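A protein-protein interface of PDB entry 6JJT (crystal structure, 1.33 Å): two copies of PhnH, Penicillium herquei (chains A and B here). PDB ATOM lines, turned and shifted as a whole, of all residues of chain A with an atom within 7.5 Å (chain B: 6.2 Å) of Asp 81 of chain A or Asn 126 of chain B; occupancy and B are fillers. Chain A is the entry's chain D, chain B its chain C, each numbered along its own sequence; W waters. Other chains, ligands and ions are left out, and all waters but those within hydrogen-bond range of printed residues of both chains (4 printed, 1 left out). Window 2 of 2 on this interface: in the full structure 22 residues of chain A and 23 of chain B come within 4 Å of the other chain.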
ATOM      1  N   ASP A  46      -4.645  16.964 -37.783  1.00  0.00           N
ATOM      2  CA  ASP A  46      -3.668  15.995 -37.297  1.00  0.00           C
ATOM      3  C   ASP A  46      -3.341  16.253 -35.827  1.00  0.00           C
ATOM      4  O   ASP A  46      -3.107  15.316 -35.077  1.00  0.00           O
ATOM      5  CB  ASP A  46      -2.361  15.929 -38.095  1.00  0.00           C
ATOM      6  CG  ASP A  46      -1.596  14.632 -37.837  1.00  0.00           C
ATOM      7  OD1 ASP A  46      -2.076  13.559 -38.308  1.00  0.00           O
ATOM      8  OD2 ASP A  46      -0.554  14.681 -37.142  1.00  0.00           O
ATOM      9  N   ALA A  47      -3.307  17.534 -35.446  1.00  0.00           N
ATOM     10  CA  ALA A  47      -2.877  17.953 -34.117  1.00  0.00           C
ATOM     11  C   ALA A  47      -3.893  17.611 -33.013  1.00  0.00           C
ATOM     12  O   ALA A  47      -3.453  17.328 -31.885  1.00  0.00           O
ATOM     13  CB  ALA A  47      -2.601  19.440 -34.137  1.00  0.00           C
ATOM     14  N   GLN A  48      -5.227  17.712 -33.302  1.00  0.00           N
ATOM     15  CA  GLN A  48      -6.237  17.472 -32.279  1.00  0.00           C
ATOM     16  C   GLN A  48      -7.664  17.362 -32.830  1.00  0.00           C
ATOM     17  O   GLN A  48      -7.916  17.781 -33.960  1.00  0.00           O
ATOM     18  CB  GLN A  48      -6.184  18.579 -31.226  1.00  0.00           C
ATOM     19  CG  GLN A  48      -6.656  19.937 -31.728  1.00  0.00           C
ATOM     20  CD  GLN A  48      -5.509  20.800 -32.181  1.00  0.00           C
ATOM     21  OE1 GLN A  48      -4.441  20.807 -31.554  1.00  0.00           O
ATOM     22  NE2 GLN A  48      -5.695  21.569 -33.245  1.00  0.00           N
ATOM     23  N   THR A  77     -10.850  18.940 -26.067  1.00  0.00           N
ATOM     24  CA  THR A  77      -9.862  18.758 -27.129  1.00  0.00           C
ATOM     25  C   THR A  77      -9.021  17.513 -26.847  1.00  0.00           C
ATOM     26  O   THR A  77      -8.386  17.456 -25.769  1.00  0.00           O
ATOM     27  CB  THR A  77      -8.905  19.949 -27.193  1.00  0.00           C
ATOM     28  OG1 THR A  77      -9.658  21.092 -27.589  1.00  0.00           O
ATOM     29  CG2 THR A  77      -7.806  19.769 -28.229  1.00  0.00           C
ATOM     30  N   ARG A  78      -9.044  16.583 -27.789  1.00  0.00           N
ATOM     31  CA  ARG A  78      -8.175  15.415 -27.722  1.00  0.00           C
ATOM     32  C   ARG A  78      -7.005  15.684 -28.650  1.00  0.00           C
ATOM     33  O   ARG A  78      -7.217  15.776 -29.851  1.00  0.00           O
ATOM     34  CB  ARG A  78      -8.933  14.191 -28.234  1.00  0.00           C
ATOM     35  CG  ARG A  78      -8.069  12.931 -28.133  1.00  0.00           C
ATOM     36  CD  ARG A  78      -8.577  11.635 -28.737  1.00  0.00           C
ATOM     37  NE  ARG A  78      -9.692  11.027 -28.018  1.00  0.00           N
ATOM     38  CZ  ARG A  78      -9.562  10.186 -26.992  1.00  0.00           C
ATOM     39  NH1 ARG A  78     -10.640   9.685 -26.408  1.00  0.00           N
ATOM     40  NH2 ARG A  78      -8.358   9.851 -26.554  1.00  0.00           N
ATOM     41  N   GLY A  79      -5.768  15.769 -28.116  1.00  0.00           N
ATOM     42  CA  GLY A  79      -4.612  16.071 -28.969  1.00  0.00           C
ATOM     43  C   GLY A  79      -4.043  14.781 -29.563  1.00  0.00           C
ATOM     44  O   GLY A  79      -4.320  13.692 -29.055  1.00  0.00           O
ATOM     45  N   ALA A  80      -3.250  14.932 -30.647  1.00  0.00           N
ATOM     46  CA  ALA A  80      -2.496  13.828 -31.237  1.00  0.00           C
ATOM     47  C   ALA A  80      -1.557  13.208 -30.197  1.00  0.00           C
ATOM     48  O   ALA A  80      -1.197  12.030 -30.295  1.00  0.00           O
ATOM     49  CB  ALA A  80      -1.721  14.303 -32.442  1.00  0.00           C
ATOM     50  N   ASP A  81      -1.154  14.014 -29.193  1.00  0.00           N
ATOM     51  CA  ASP A  81      -0.236  13.583 -28.146  1.00  0.00           C
ATOM     52  C   ASP A  81      -0.934  12.704 -27.114  1.00  0.00           C
ATOM     53  O   ASP A  81      -0.257  12.234 -26.201  1.00  0.00           O
ATOM     54  CB  ASP A  81       0.440  14.780 -27.476  1.00  0.00           C
ATOM     55  CG  ASP A  81      -0.472  15.630 -26.608  1.00  0.00           C
ATOM     56  OD1 ASP A  81      -1.713  15.459 -26.689  1.00  0.00           O
ATOM     57  OD2 ASP A  81       0.078  16.496 -25.903  1.00  0.00           O
ATOM     58  N   GLY A  82      -2.260  12.512 -27.228  1.00  0.00           N
ATOM     59  CA  GLY A  82      -2.964  11.652 -26.289  1.00  0.00           C
ATOM     60  C   GLY A  82      -3.646  12.396 -25.131  1.00  0.00           C
ATOM     61  O   GLY A  82      -4.360  11.779 -24.342  1.00  0.00           O
ATOM     62  N   THR A  83      -3.372  13.684 -24.953  1.00  0.00           N
ATOM     63  CA  THR A  83      -3.976  14.401 -23.838  1.00  0.00           C
ATOM     64  C   THR A  83      -5.448  14.687 -24.194  1.00  0.00           C
ATOM     65  O   THR A  83      -5.736  15.022 -25.350  1.00  0.00           O
ATOM     66  CB  THR A  83      -3.251  15.740 -23.632  1.00  0.00           C
ATOM     67  OG1 THR A  83      -1.837  15.490 -23.628  1.00  0.00           O
ATOM     68  CG2 THR A  83      -3.669  16.501 -22.390  1.00  0.00           C
ATOM     69  N   ILE A  84      -6.370  14.654 -23.220  1.00  0.00           N
ATOM     70  CA  ILE A  84      -7.739  15.122 -23.416  1.00  0.00           C
ATOM     71  C   ILE A  84      -8.033  16.228 -22.409  1.00  0.00           C
ATOM     72  O   ILE A  84      -8.084  15.999 -21.178  1.00  0.00           O
ATOM     73  CB  ILE A  84      -8.747  13.985 -23.211  1.00  0.00           C
ATOM     74  CG1 ILE A  84      -8.437  12.759 -24.087  1.00  0.00           C
ATOM     75  CG2 ILE A  84     -10.120  14.556 -23.480  1.00  0.00           C
ATOM     76  CD1 ILE A  84      -9.154  11.473 -23.653  1.00  0.00           C
ATOM     77  N   ARG A  85      -8.162  17.469 -22.891  1.00  0.00           N
ATOM     78  CA  ARG A  85      -8.432  18.599 -22.017  1.00  0.00           C
ATOM     79  C   ARG A  85      -9.916  18.963 -22.144  1.00  0.00           C
ATOM     80  O   ARG A  85     -10.462  18.889 -23.257  1.00  0.00           O
ATOM     81  CB  ARG A  85      -7.571  19.779 -22.442  1.00  0.00           C
ATOM     82  CG  ARG A  85      -6.077  19.564 -22.222  1.00  0.00           C
ATOM     83  CD  ARG A  85      -5.313  20.845 -22.381  1.00  0.00           C
ATOM     84  NE  ARG A  85      -3.909  20.612 -21.960  1.00  0.00           N
ATOM     85  CZ  ARG A  85      -2.919  20.207 -22.757  1.00  0.00           C
ATOM     86  NH1 ARG A  85      -1.734  20.002 -22.217  1.00  0.00           N
ATOM     87  NH2 ARG A  85      -3.128  19.918 -24.030  1.00  0.00           N
ATOM     88  N   ALA A 106     -10.308  20.124 -16.829  1.00  0.00           N
ATOM     89  CA  ALA A 106      -9.943  18.722 -16.654  1.00  0.00           C
ATOM     90  C   ALA A 106      -8.795  18.323 -17.545  1.00  0.00           C
ATOM     91  O   ALA A 106      -8.740  18.744 -18.682  1.00  0.00           O
ATOM     92  CB  ALA A 106     -11.149  17.834 -16.939  1.00  0.00           C
ATOM     93  N   ALA A 107      -7.875  17.497 -17.006  1.00  0.00           N
ATOM     94  CA  ALA A 107      -7.010  16.645 -17.795  1.00  0.00           C
ATOM     95  C   ALA A 107      -7.608  15.256 -17.683  1.00  0.00           C
ATOM     96  O   ALA A 107      -7.361  14.536 -16.702  1.00  0.00           O
ATOM     97  CB  ALA A 107      -5.589  16.698 -17.232  1.00  0.00           C
ATOM     98  N   ILE A 108      -8.545  14.953 -18.583  1.00  0.00           N
ATOM     99  CA  ILE A 108      -9.429  13.810 -18.394  1.00  0.00           C
ATOM    100  C   ILE A 108      -8.553  12.580 -18.143  1.00  0.00           C
ATOM    101  O   ILE A 108      -7.568  12.344 -18.838  1.00  0.00           O
ATOM    102  CB  ILE A 108     -10.306  13.664 -19.666  1.00  0.00           C
ATOM    103  CG1 ILE A 108     -11.335  14.799 -19.826  1.00  0.00           C
ATOM    104  CG2 ILE A 108     -10.981  12.282 -19.836  1.00  0.00           C
ATOM    105  CD1 ILE A 108     -12.425  14.804 -18.793  1.00  0.00           C
ATOM    106  N   LEU B 114      -3.273  23.447 -14.039  1.00  0.00           N
ATOM    107  CA  LEU B 114      -3.180  22.621 -15.236  1.00  0.00           C
ATOM    108  C   LEU B 114      -1.951  23.022 -16.042  1.00  0.00           C
ATOM    109  O   LEU B 114      -1.460  24.149 -15.857  1.00  0.00           O
ATOM    110  CB  LEU B 114      -4.441  22.803 -16.091  1.00  0.00           C
ATOM    111  CG  LEU B 114      -5.705  22.231 -15.453  1.00  0.00           C
ATOM    112  CD1 LEU B 114      -6.943  22.765 -16.184  1.00  0.00           C
ATOM    113  CD2 LEU B 114      -5.738  20.705 -15.430  1.00  0.00           C
ATOM    114  N   PHE B 115      -1.472  22.151 -16.902  1.00  0.00           N
ATOM    115  CA  PHE B 115      -0.202  22.344 -17.589  1.00  0.00           C
ATOM    116  C   PHE B 115      -0.297  22.027 -19.074  1.00  0.00           C
ATOM    117  O   PHE B 115      -1.076  21.170 -19.506  1.00  0.00           O
ATOM    118  CB  PHE B 115       0.865  21.375 -17.025  1.00  0.00           C
ATOM    119  CG  PHE B 115       1.132  21.579 -15.557  1.00  0.00           C
ATOM    120  CD1 PHE B 115       2.027  22.567 -15.110  1.00  0.00           C
ATOM    121  CD2 PHE B 115       0.492  20.780 -14.614  1.00  0.00           C
ATOM    122  CE1 PHE B 115       2.277  22.734 -13.752  1.00  0.00           C
ATOM    123  CE2 PHE B 115       0.743  20.970 -13.263  1.00  0.00           C
ATOM    124  CZ  PHE B 115       1.631  21.943 -12.832  1.00  0.00           C
ATOM    125  N   ASP B 116       0.581  22.659 -19.845  1.00  0.00           N
ATOM    126  CA  ASP B 116       0.677  22.294 -21.247  1.00  0.00           C
ATOM    127  C   ASP B 116       2.128  22.445 -21.687  1.00  0.00           C
ATOM    128  O   ASP B 116       2.725  23.518 -21.584  1.00  0.00           O
ATOM    129  CB  ASP B 116      -0.269  23.180 -22.088  1.00  0.00           C
ATOM    130  CG  ASP B 116      -0.417  22.723 -23.530  1.00  0.00           C
ATOM    131  OD1 ASP B 116       0.586  22.146 -24.078  1.00  0.00           O
ATOM    132  OD2 ASP B 116      -1.504  22.951 -24.153  1.00  0.00           O
ATOM    133  N   THR B 117       2.725  21.309 -22.114  1.00  0.00           N
ATOM    134  CA  THR B 117       4.051  21.325 -22.713  1.00  0.00           C
ATOM    135  C   THR B 117       4.203  20.187 -23.708  1.00  0.00           C
ATOM    136  O   THR B 117       3.832  19.051 -23.352  1.00  0.00           O
ATOM    137  CB  THR B 117       5.164  21.210 -21.658  1.00  0.00           C
ATOM    138  OG1 THR B 117       6.398  21.396 -22.354  1.00  0.00           O
ATOM    139  CG2 THR B 117       5.217  19.880 -20.917  1.00  0.00           C
ATOM    140  N   SER B 118       4.803  20.414 -24.862  1.00  0.00           N
ATOM    141  CA  SER B 118       5.139  19.343 -25.791  1.00  0.00           C
ATOM    142  C   SER B 118       6.565  18.846 -25.545  1.00  0.00           C
ATOM    143  O   SER B 118       6.985  17.938 -26.249  1.00  0.00           O
ATOM    144  CB  SER B 118       4.907  19.796 -27.201  1.00  0.00           C
ATOM    145  OG  SER B 118       5.703  20.870 -27.538  1.00  0.00           O
ATOM    146  N   TYR B 122       9.023  16.408 -20.404  1.00  0.00           N
ATOM    147  CA  TYR B 122       8.106  16.830 -19.362  1.00  0.00           C
ATOM    148  C   TYR B 122       6.647  16.663 -19.801  1.00  0.00           C
ATOM    149  O   TYR B 122       5.777  17.132 -19.103  1.00  0.00           O
ATOM    150  CB  TYR B 122       8.392  18.282 -18.915  1.00  0.00           C
ATOM    151  CG  TYR B 122       9.826  18.480 -18.491  1.00  0.00           C
ATOM    152  CD1 TYR B 122      10.333  17.811 -17.365  1.00  0.00           C
ATOM    153  CD2 TYR B 122      10.686  19.241 -19.267  1.00  0.00           C
ATOM    154  CE1 TYR B 122      11.655  17.984 -16.991  1.00  0.00           C
ATOM    155  CE2 TYR B 122      12.035  19.354 -18.950  1.00  0.00           C
ATOM    156  CZ  TYR B 122      12.498  18.725 -17.807  1.00  0.00           C
ATOM    157  OH  TYR B 122      13.820  18.841 -17.426  1.00  0.00           O
ATOM    158  N   ASN B 123       6.383  16.004 -20.930  1.00  0.00           N
ATOM    159  CA  ASN B 123       5.021  16.003 -21.448  1.00  0.00           C
ATOM    160  C   ASN B 123       4.045  15.195 -20.576  1.00  0.00           C
ATOM    161  O   ASN B 123       2.851  15.277 -20.804  1.00  0.00           O
ATOM    162  CB  ASN B 123       5.003  15.625 -22.920  1.00  0.00           C
ATOM    163  CG  ASN B 123       5.436  14.201 -23.160  1.00  0.00           C
ATOM    164  OD1 ASN B 123       5.384  13.366 -22.256  1.00  0.00           O
ATOM    165  ND2 ASN B 123       5.813  13.899 -24.394  1.00  0.00           N
ATOM    166  N   TRP B 124       4.513  14.432 -19.572  1.00  0.00           N
ATOM    167  CA  TRP B 124       3.626  13.814 -18.611  1.00  0.00           C
ATOM    168  C   TRP B 124       2.790  14.869 -17.886  1.00  0.00           C
ATOM    169  O   TRP B 124       1.712  14.614 -17.376  1.00  0.00           O
ATOM    170  CB  TRP B 124       4.418  12.894 -17.633  1.00  0.00           C
ATOM    171  CG  TRP B 124       5.599  13.594 -17.030  1.00  0.00           C
ATOM    172  CD1 TRP B 124       6.888  13.650 -17.494  1.00  0.00           C
ATOM    173  CD2 TRP B 124       5.567  14.436 -15.867  1.00  0.00           C
ATOM    174  NE1 TRP B 124       7.648  14.470 -16.712  1.00  0.00           N
ATOM    175  CE2 TRP B 124       6.878  14.962 -15.707  1.00  0.00           C
ATOM    176  CE3 TRP B 124       4.571  14.795 -14.956  1.00  0.00           C
ATOM    177  CZ2 TRP B 124       7.215  15.842 -14.698  1.00  0.00           C
ATOM    178  CZ3 TRP B 124       4.911  15.647 -13.934  1.00  0.00           C
ATOM    179  CH2 TRP B 124       6.216  16.140 -13.799  1.00  0.00           C
ATOM    180  N   LEU B 125       3.296  16.118 -17.836  1.00  0.00           N
ATOM    181  CA  LEU B 125       2.520  17.180 -17.174  1.00  0.00           C
ATOM    182  C   LEU B 125       1.162  17.477 -17.836  1.00  0.00           C
ATOM    183  O   LEU B 125       0.244  17.942 -17.172  1.00  0.00           O
ATOM    184  CB  LEU B 125       3.352  18.474 -17.161  1.00  0.00           C
ATOM    185  CG  LEU B 125       4.464  18.534 -16.118  1.00  0.00           C
ATOM    186  CD1 LEU B 125       5.385  19.694 -16.492  1.00  0.00           C
ATOM    187  CD2 LEU B 125       3.862  18.733 -14.734  1.00  0.00           C
ATOM    188  N   ASN B 126       1.037  17.163 -19.134  1.00  0.00           N
ATOM    189  CA  ASN B 126      -0.194  17.414 -19.871  1.00  0.00           C
ATOM    190  C   ASN B 126      -1.354  16.706 -19.221  1.00  0.00           C
ATOM    191  O   ASN B 126      -2.474  17.209 -19.261  1.00  0.00           O
ATOM    192  CB  ASN B 126      -0.074  17.009 -21.315  1.00  0.00           C
ATOM    193  CG  ASN B 126       0.904  17.875 -22.084  1.00  0.00           C
ATOM    194  OD1 ASN B 126       1.086  19.059 -21.723  1.00  0.00           O
ATOM    195  ND2 ASN B 126       1.592  17.349 -23.057  1.00  0.00           N
ATOM    196  N   ASN B 127      -1.085  15.577 -18.563  1.00  0.00           N
ATOM    197  CA  ASN B 127      -2.115  14.738 -17.982  1.00  0.00           C
ATOM    198  C   ASN B 127      -2.282  14.960 -16.486  1.00  0.00           C
ATOM    199  O   ASN B 127      -3.030  14.221 -15.822  1.00  0.00           O
ATOM    200  CB  ASN B 127      -1.830  13.265 -18.325  1.00  0.00           C
ATOM    201  CG  ASN B 127      -1.927  13.056 -19.825  1.00  0.00           C
ATOM    202  OD1 ASN B 127      -2.888  13.487 -20.495  1.00  0.00           O
ATOM    203  ND2 ASN B 127      -0.863  12.524 -20.418  1.00  0.00           N
ATOM    204  N   VAL B 128      -1.639  16.021 -15.947  1.00  0.00           N
ATOM    205  CA  VAL B 128      -1.656  16.261 -14.516  1.00  0.00           C
ATOM    206  C   VAL B 128      -2.657  17.347 -14.117  1.00  0.00           C
ATOM    207  O   VAL B 128      -2.718  18.447 -14.736  1.00  0.00           O
ATOM    208  CB  VAL B 128      -0.247  16.700 -14.049  1.00  0.00           C
ATOM    209  CG1 VAL B 128      -0.261  17.254 -12.640  1.00  0.00           C
ATOM    210  CG2 VAL B 128       0.764  15.543 -14.190  1.00  0.00           C
HETATM  211  O   HOH W   1      -5.647  14.000 -20.481  1.00  0.00           O
HETATM  212  O   HOH W   2      -0.568  18.904 -25.001  1.00  0.00           O
HETATM  213  O   HOH W   3      -4.245  20.955 -19.264  1.00  0.00           O
HETATM  214  O   HOH W   4       2.430  17.185 -26.182  1.00  0.00           O
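N of Thr 77 of chain A lies within hydrogen-bond range of O of Arg 85 of chain A (2.8 Å). ND2 of Asn 126 of chain B is in hydrogen-bond range of O of Asn 123 of chain B (3.3 Å). OD1 of Asp 81 of chain A is in hydrogen-bond range of N of Thr 83 of chain A (3.0 Å). The side-chain amide oxygen (OD1) of Asn 126 of chain B lies within hydrogen-bond range of the backbone NH (N) of Thr 117 of chain B.
Among the printed residues, merely in contact across the chains: Thr 83 of chain A with Asn 126 of chain B, Thr 83 of chain A with Asn 127 of chain B, Ala 107 of chain A with Asn 126 of chain B and Ala 107 of chain A with Asn 127 of chain B.
No position is printed for both chains.
Of the 12 printed residues of chain B, 4 touch a printed residue of chain A. Along chain B the printed residues that touch a printed residue of chain A span positions 115 to 127. Hydrophobic or aromatic side chains of chain A that line the printed part of chain B: Ala 107. Among the printed residues, 8 pairs touch across the chains. Among the printed residues, Asp or Glu carboxylates within 4 Å of a Lys or Arg side-chain nitrogen of the other chain: Arg 85 of chain A with Asp 116 of chain B (3.4 Å).
The guanidinium group of Arg 85 of chain A is in salt-bridge range of the side-chain carboxylate of Asp 116 of chain B (3.4 Å). The guanidinium group (NH1) of Arg 85 of chain A sits at hydrogen-bond distance from the backbone carbonyl oxygen (O) of Phe 115 of chain B, at 3.0 Å. ND2 of Asn 126 of chain B is in hydrogen-bond range of OD2 of Asp 81 of chain A, at 3.3 Å. The side-chain amide oxygen (OD1) of Asn 126 of chain B lies within hydrogen-bond range of the guanidinium group (NH1) of Arg 85 of chain A (3.0 Å).
Of chain B, only Asn 126 comes within 4 Å of Asp 81 of chain A. Printed residues of chain B within 4 Å of Arg 85 of chain A: Phe 115 (3.0 Å), Asp 116 (3.3 Å) and Asn 126 (3.0 Å). Leu 114 of chain B touches none of the printed residues of chain A. Printed residues of chain A within 4 Å of Phe 115 of chain B: Arg 85. Printed residues of chain A within 4 Å of Asp 116 of chain B: Arg 85 (3.3 Å). Thr 117 of chain B touches none of the printed residues of chain A. Of the printed residues of chain A, Asn 127 of chain B touches Thr 83 (3.6 Å) and Ala 107 (3.8 Å). The nearest printed residue of chain B that does not touch Thr 83 of chain A is Asn 123 of chain B (5.5 Å).
Water W4 lies within hydrogen-bond range of OD2 of Asp 81 of chain A and ND2 of Asn 126 of chain B. Water W2 lies within hydrogen-bond range of OD2 of Asp 81 of chain A, NH2 of Arg 85 of chain A and ND2 of Asn 126 of chain B. Water W3 lies within hydrogen-bond range of the guanidinium group (NE) of Arg 85 of chain A (2.7 Å) and the backbone carbonyl oxygen (O) of Phe 115 of chain B (3.2 Å). Water W1 lies within hydrogen-bond range of OD1 of Asn 127 of chain B (2.8 Å), N of Ile 84 of chain A (2.9 Å) and O of Ile 108 of chain A (3.0 Å).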
